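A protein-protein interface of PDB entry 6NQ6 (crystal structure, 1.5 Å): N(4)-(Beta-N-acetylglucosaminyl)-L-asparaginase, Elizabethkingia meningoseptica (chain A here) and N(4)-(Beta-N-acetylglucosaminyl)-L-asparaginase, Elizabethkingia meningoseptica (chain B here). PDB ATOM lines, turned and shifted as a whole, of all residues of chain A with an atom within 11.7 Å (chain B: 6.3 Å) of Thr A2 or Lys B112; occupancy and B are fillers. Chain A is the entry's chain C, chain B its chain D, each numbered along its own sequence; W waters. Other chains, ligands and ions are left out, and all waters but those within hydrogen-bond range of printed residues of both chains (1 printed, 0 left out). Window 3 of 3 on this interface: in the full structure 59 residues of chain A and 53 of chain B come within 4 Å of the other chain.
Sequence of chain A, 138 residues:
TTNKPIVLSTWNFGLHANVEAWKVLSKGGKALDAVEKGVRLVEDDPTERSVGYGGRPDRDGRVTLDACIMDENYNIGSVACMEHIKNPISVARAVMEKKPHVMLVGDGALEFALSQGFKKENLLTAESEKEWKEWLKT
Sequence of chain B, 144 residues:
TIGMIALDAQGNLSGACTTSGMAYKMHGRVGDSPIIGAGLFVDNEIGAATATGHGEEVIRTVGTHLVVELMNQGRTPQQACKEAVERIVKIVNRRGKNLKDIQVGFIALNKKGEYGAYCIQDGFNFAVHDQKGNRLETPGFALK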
ATOM      1  N   THR A   2     -14.873 -13.773 -24.229  1.00  0.00           N
ATOM      2  CA  THR A   2     -14.509 -15.060 -23.561  1.00  0.00           C
ATOM      3  C   THR A   2     -13.327 -14.920 -22.594  1.00  0.00           C
ATOM      4  O   THR A   2     -12.258 -14.391 -22.954  1.00  0.00           O
ATOM      5  CB  THR A   2     -14.143 -16.153 -24.576  1.00  0.00           C
ATOM      6  OG1 THR A   2     -15.283 -16.419 -25.432  1.00  0.00           O
ATOM      7  CG2 THR A   2     -13.718 -17.481 -23.878  1.00  0.00           C
ATOM      8  N   ASN A   3     -13.479 -15.455 -21.382  1.00  0.00           N
ATOM      9  CA  ASN A   3     -12.425 -15.452 -20.404  1.00  0.00           C
ATOM     10  C   ASN A   3     -11.723 -16.818 -20.355  1.00  0.00           C
ATOM     11  O   ASN A   3     -12.310 -17.739 -19.802  1.00  0.00           O
ATOM     12  CB  ASN A   3     -13.000 -15.142 -19.036  1.00  0.00           C
ATOM     13  CG  ASN A   3     -11.928 -14.966 -17.970  1.00  0.00           C
ATOM     14  OD1 ASN A   3     -10.776 -14.880 -18.268  1.00  0.00           O
ATOM     15  ND2 ASN A   3     -12.333 -14.921 -16.709  1.00  0.00           N
ATOM     16  N   LYS A   4     -10.623 -16.968 -21.070  1.00  0.00           N
ATOM     17  CA  LYS A   4      -9.954 -18.254 -21.162  1.00  0.00           C
ATOM     18  C   LYS A   4      -8.463 -18.057 -21.275  1.00  0.00           C
ATOM     19  O   LYS A   4      -7.998 -17.043 -21.858  1.00  0.00           O
ATOM     20  CB  LYS A   4     -10.477 -19.087 -22.348  1.00  0.00           C
ATOM     21  CG  LYS A   4     -10.088 -18.583 -23.729  1.00  0.00           C
ATOM     22  CD  LYS A   4     -10.736 -19.486 -24.812  1.00  0.00           C
ATOM     23  CE  LYS A   4     -10.742 -18.888 -26.241  1.00  0.00           C
ATOM     24  NZ  LYS A   4      -9.342 -18.716 -26.654  1.00  0.00           N
ATOM     25  N   PRO A   5      -7.662 -18.977 -20.801  1.00  0.00           N
ATOM     26  CA  PRO A   5      -8.046 -20.140 -20.021  1.00  0.00           C
ATOM     27  C   PRO A   5      -8.464 -19.776 -18.632  1.00  0.00           C
ATOM     28  O   PRO A   5      -8.170 -18.656 -18.120  1.00  0.00           O
ATOM     29  CB  PRO A   5      -6.754 -20.986 -19.970  1.00  0.00           C
ATOM     30  CG  PRO A   5      -5.667 -20.216 -20.599  1.00  0.00           C
ATOM     31  CD  PRO A   5      -6.220 -18.892 -20.994  1.00  0.00           C
ATOM     32  N   ILE A   6      -9.206 -20.708 -17.990  1.00  0.00           N
ATOM     33  CA  ILE A   6      -9.704 -20.495 -16.634  1.00  0.00           C
ATOM     34  C   ILE A   6      -9.899 -21.906 -15.983  1.00  0.00           C
ATOM     35  O   ILE A   6     -10.277 -22.858 -16.666  1.00  0.00           O
ATOM     36  CB  ILE A   6     -10.992 -19.665 -16.637  1.00  0.00           C
ATOM     37  CG1 ILE A   6     -11.607 -19.477 -15.233  1.00  0.00           C
ATOM     38  CG2 ILE A   6     -12.065 -20.199 -17.551  1.00  0.00           C
ATOM     39  CD1 ILE A   6     -12.629 -18.363 -15.055  1.00  0.00           C
ATOM     40  N   VAL A   7      -9.651 -21.975 -14.672  1.00  0.00           N
ATOM     41  CA  VAL A   7      -9.836 -23.199 -13.933  1.00  0.00           C
ATOM     42  C   VAL A   7     -10.506 -22.843 -12.646  1.00  0.00           C
ATOM     43  O   VAL A   7     -10.119 -21.849 -11.970  1.00  0.00           O
ATOM     44  CB  VAL A   7      -8.518 -23.949 -13.728  1.00  0.00           C
ATOM     45  CG1 VAL A   7      -7.474 -23.047 -13.081  1.00  0.00           C
ATOM     46  CG2 VAL A   7      -8.707 -25.247 -12.912  1.00  0.00           C
ATOM     47  N   LEU A   8     -11.459 -23.694 -12.249  1.00  0.00           N
ATOM     48  CA  LEU A   8     -12.178 -23.662 -10.917  1.00  0.00           C
ATOM     49  C   LEU A   8     -12.000 -24.924 -10.186  1.00  0.00           C
ATOM     50  O   LEU A   8     -12.013 -26.024 -10.806  1.00  0.00           O
ATOM     51  CB  LEU A   8     -13.691 -23.373 -11.067  1.00  0.00           C
ATOM     52  CG  LEU A   8     -14.138 -21.919 -11.227  1.00  0.00           C
ATOM     53  CD1 LEU A   8     -13.740 -21.372 -12.581  1.00  0.00           C
ATOM     54  CD2 LEU A   8     -15.634 -21.981 -11.071  1.00  0.00           C
ATOM     55  N   TRP A  22      -2.671 -24.369 -13.731  1.00  0.00           N
ATOM     56  CA  TRP A  22      -2.280 -23.231 -14.495  1.00  0.00           C
ATOM     57  C   TRP A  22      -0.924 -23.415 -15.181  1.00  0.00           C
ATOM     58  O   TRP A  22      -0.720 -22.821 -16.238  1.00  0.00           O
ATOM     59  CB  TRP A  22      -2.281 -21.922 -13.665  1.00  0.00           C
ATOM     60  CG  TRP A  22      -2.347 -20.664 -14.436  1.00  0.00           C
ATOM     61  CD1 TRP A  22      -1.319 -19.755 -14.589  1.00  0.00           C
ATOM     62  CD2 TRP A  22      -3.435 -20.142 -15.171  1.00  0.00           C
ATOM     63  NE1 TRP A  22      -1.700 -18.737 -15.388  1.00  0.00           N
ATOM     64  CE2 TRP A  22      -3.007 -18.906 -15.743  1.00  0.00           C
ATOM     65  CE3 TRP A  22      -4.718 -20.586 -15.430  1.00  0.00           C
ATOM     66  CZ2 TRP A  22      -3.783 -18.182 -16.564  1.00  0.00           C
ATOM     67  CZ3 TRP A  22      -5.513 -19.844 -16.220  1.00  0.00           C
ATOM     68  CH2 TRP A  22      -5.057 -18.626 -16.779  1.00  0.00           C
ATOM     69  N   LEU B   7     -11.473 -24.565 -18.629  1.00  0.00           N
ATOM     70  CA  LEU B   7     -11.628 -24.158 -20.037  1.00  0.00           C
ATOM     71  C   LEU B   7     -10.265 -23.715 -20.529  1.00  0.00           C
ATOM     72  O   LEU B   7      -9.652 -22.750 -20.001  1.00  0.00           O
ATOM     73  CB  LEU B   7     -12.583 -22.989 -20.113  1.00  0.00           C
ATOM     74  CG  LEU B   7     -12.892 -22.340 -21.492  1.00  0.00           C
ATOM     75  CD1 LEU B   7     -13.680 -23.246 -22.392  1.00  0.00           C
ATOM     76  CD2 LEU B   7     -13.765 -21.091 -21.285  1.00  0.00           C
ATOM     77  N   GLY B  11     -10.627 -23.273 -26.079  1.00  0.00           N
ATOM     78  CA  GLY B  11     -12.046 -23.200 -25.837  1.00  0.00           C
ATOM     79  C   GLY B  11     -12.713 -24.550 -25.489  1.00  0.00           C
ATOM     80  O   GLY B  11     -13.930 -24.690 -25.571  1.00  0.00           O
ATOM     81  N   ILE B  46     -21.744 -26.529 -23.995  1.00  0.00           N
ATOM     82  CA  ILE B  46     -22.495 -25.805 -22.968  1.00  0.00           C
ATOM     83  C   ILE B  46     -21.652 -25.344 -21.780  1.00  0.00           C
ATOM     84  O   ILE B  46     -21.626 -24.170 -21.495  1.00  0.00           O
ATOM     85  CB  ILE B  46     -23.654 -26.652 -22.418  1.00  0.00           C
ATOM     86  CG1 ILE B  46     -24.603 -27.127 -23.553  1.00  0.00           C
ATOM     87  CG2 ILE B  46     -24.368 -25.898 -21.295  1.00  0.00           C
ATOM     88  CD1 ILE B  46     -25.451 -28.293 -23.164  1.00  0.00           C
ATOM     89  N   ASN B 110     -19.134 -21.877 -18.035  1.00  0.00           N
ATOM     90  CA  ASN B 110     -19.732 -22.040 -19.363  1.00  0.00           C
ATOM     91  C   ASN B 110     -18.623 -21.869 -20.426  1.00  0.00           C
ATOM     92  O   ASN B 110     -17.458 -21.613 -20.129  1.00  0.00           O
ATOM     93  CB  ASN B 110     -20.985 -21.172 -19.556  1.00  0.00           C
ATOM     94  CG  ASN B 110     -20.680 -19.686 -19.659  1.00  0.00           C
ATOM     95  OD1 ASN B 110     -19.551 -19.290 -19.877  1.00  0.00           O
ATOM     96  ND2 ASN B 110     -21.737 -18.846 -19.509  1.00  0.00           N
ATOM     97  N   LYS B 111     -19.020 -22.058 -21.680  1.00  0.00           N
ATOM     98  CA  LYS B 111     -18.103 -21.958 -22.809  1.00  0.00           C
ATOM     99  C   LYS B 111     -17.376 -20.621 -22.845  1.00  0.00           C
ATOM    100  O   LYS B 111     -16.183 -20.561 -23.143  1.00  0.00           O
ATOM    101  CB  LYS B 111     -18.850 -22.182 -24.125  1.00  0.00           C
ATOM    102  CG  LYS B 111     -19.390 -23.592 -24.299  1.00  0.00           C
ATOM    103  CD  LYS B 111     -18.263 -24.606 -24.412  1.00  0.00           C
ATOM    104  CE  LYS B 111     -17.512 -24.454 -25.724  1.00  0.00           C
ATOM    105  NZ  LYS B 111     -16.470 -25.504 -25.893  1.00  0.00           N
ATOM    106  N   LYS B 112     -18.097 -19.548 -22.539  1.00  0.00           N
ATOM    107  CA  LYS B 112     -17.504 -18.216 -22.549  1.00  0.00           C
ATOM    108  C   LYS B 112     -16.559 -17.922 -21.384  1.00  0.00           C
ATOM    109  O   LYS B 112     -16.071 -16.876 -21.279  1.00  0.00           O
ATOM    110  CB  LYS B 112     -18.628 -17.179 -22.567  1.00  0.00           C
ATOM    111  CG  LYS B 112     -19.427 -17.248 -23.851  1.00  0.00           C
ATOM    112  CD  LYS B 112     -18.487 -17.115 -25.049  1.00  0.00           C
ATOM    113  CE  LYS B 112     -18.724 -18.113 -26.193  1.00  0.00           C
ATOM    114  NZ  LYS B 112     -17.594 -19.044 -26.520  1.00  0.00           N
ATOM    115  N   GLY B 113     -16.357 -18.887 -20.494  1.00  0.00           N
ATOM    116  CA  GLY B 113     -15.511 -18.600 -19.389  1.00  0.00           C
ATOM    117  C   GLY B 113     -16.179 -17.889 -18.244  1.00  0.00           C
ATOM    118  O   GLY B 113     -15.486 -17.551 -17.328  1.00  0.00           O
ATOM    119  N   GLU B 114     -17.500 -17.631 -18.326  1.00  0.00           N
ATOM    120  CA  GLU B 114     -18.266 -17.172 -17.187  1.00  0.00           C
ATOM    121  C   GLU B 114     -18.226 -18.298 -16.158  1.00  0.00           C
ATOM    122  O   GLU B 114     -18.216 -19.455 -16.515  1.00  0.00           O
ATOM    123  CB  GLU B 114     -19.668 -16.792 -17.539  1.00  0.00           C
ATOM    124  CG  GLU B 114     -19.678 -15.470 -18.286  1.00  0.00           C
ATOM    125  CD  GLU B 114     -20.747 -15.289 -19.340  1.00  0.00           C
ATOM    126  OE1 GLU B 114     -21.691 -16.120 -19.512  1.00  0.00           O
ATOM    127  OE2 GLU B 114     -20.601 -14.255 -20.059  1.00  0.00           O
HETATM  128  O   HOH W   1     -15.278 -15.072 -16.287  1.00  0.00           O
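The backbone carbonyl oxygen (O) of Ile A6 sits at hydrogen-bond distance from the backbone NH (N) of Leu B7, at 2.9 Å.
N of Asn A3 sits at hydrogen-bond distance from O of Lys B112 (3.0 Å).
The backbone carbonyl oxygen of Gly B11 sits at hydrogen-bond distance from the side-chain amino group of Lys B111.
The side-chain amide oxygen of Asn B110 lies within hydrogen-bond range of the backbone NH of Gly B113 (3.3 Å).
The side-chain amide oxygen of Asn B110 lies within hydrogen-bond range of the backbone NH of Lys B112, 3.0 Å away.
Among the printed residues, pairs that only touch across the chains: Pro A5 with Leu B7 (3.1 Å), Thr A2 with Lys B112 (3.3 Å), Asn A3 with Gly B113 (3.3 Å), Ile A6 with Gly B113 (3.7 Å), Asn A3 with Leu B7 (3.9 Å), Lys A4 with Leu B7 (3.99 Å) and Lys A4 with Gly B11 (3.99 Å).
Printed residues of chain B within 4 Å of Thr A2: Lys B112.
Of the printed residues of chain B, Asn A3 touches Leu B7 (3.9 Å), Lys B112 (3.0 Å) and Gly B113 (3.3 Å).
Of the printed residues of chain B, Ile A6 touches Leu B7 (2.9 Å) and Gly B113 (3.7 Å).
Trp A22 touches none of the printed residues of chain B.
No residue of chain A comes within 4 Å of Asn B110.
Of chain A, only Thr A2 (3.3 Å) and Asn A3 (3.0 Å) come within 4 Å of Lys B112.
Of chain A, only Asn A3 and Ile A6 come within 4 Å of Gly B113.
No residue of chain A comes within 4 Å of Glu B114.
The nearest printed residue of chain B that does not touch Thr A2 is Lys B111 (4.01 Å).
The nearest printed residue of chain A that does not touch Leu B7 is Thr A2 (4.4 Å).
Of the 8 printed residues of chain A, 5 touch a printed residue of chain B.
Hydrophobic or aromatic side chains of chain A that line the printed part of chain B: Pro A5 and Ile A6.
Among the printed residues, 9 pairs touch across the chains.
Among the printed residues, no Asp or Glu carboxylate lies within 4 Å of a Lys or Arg side-chain nitrogen of the other chain.
Water W1 lies within hydrogen-bond range of O of Gly B113 (2.7 Å) and ND2 of Asn A3 (3.0 Å).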
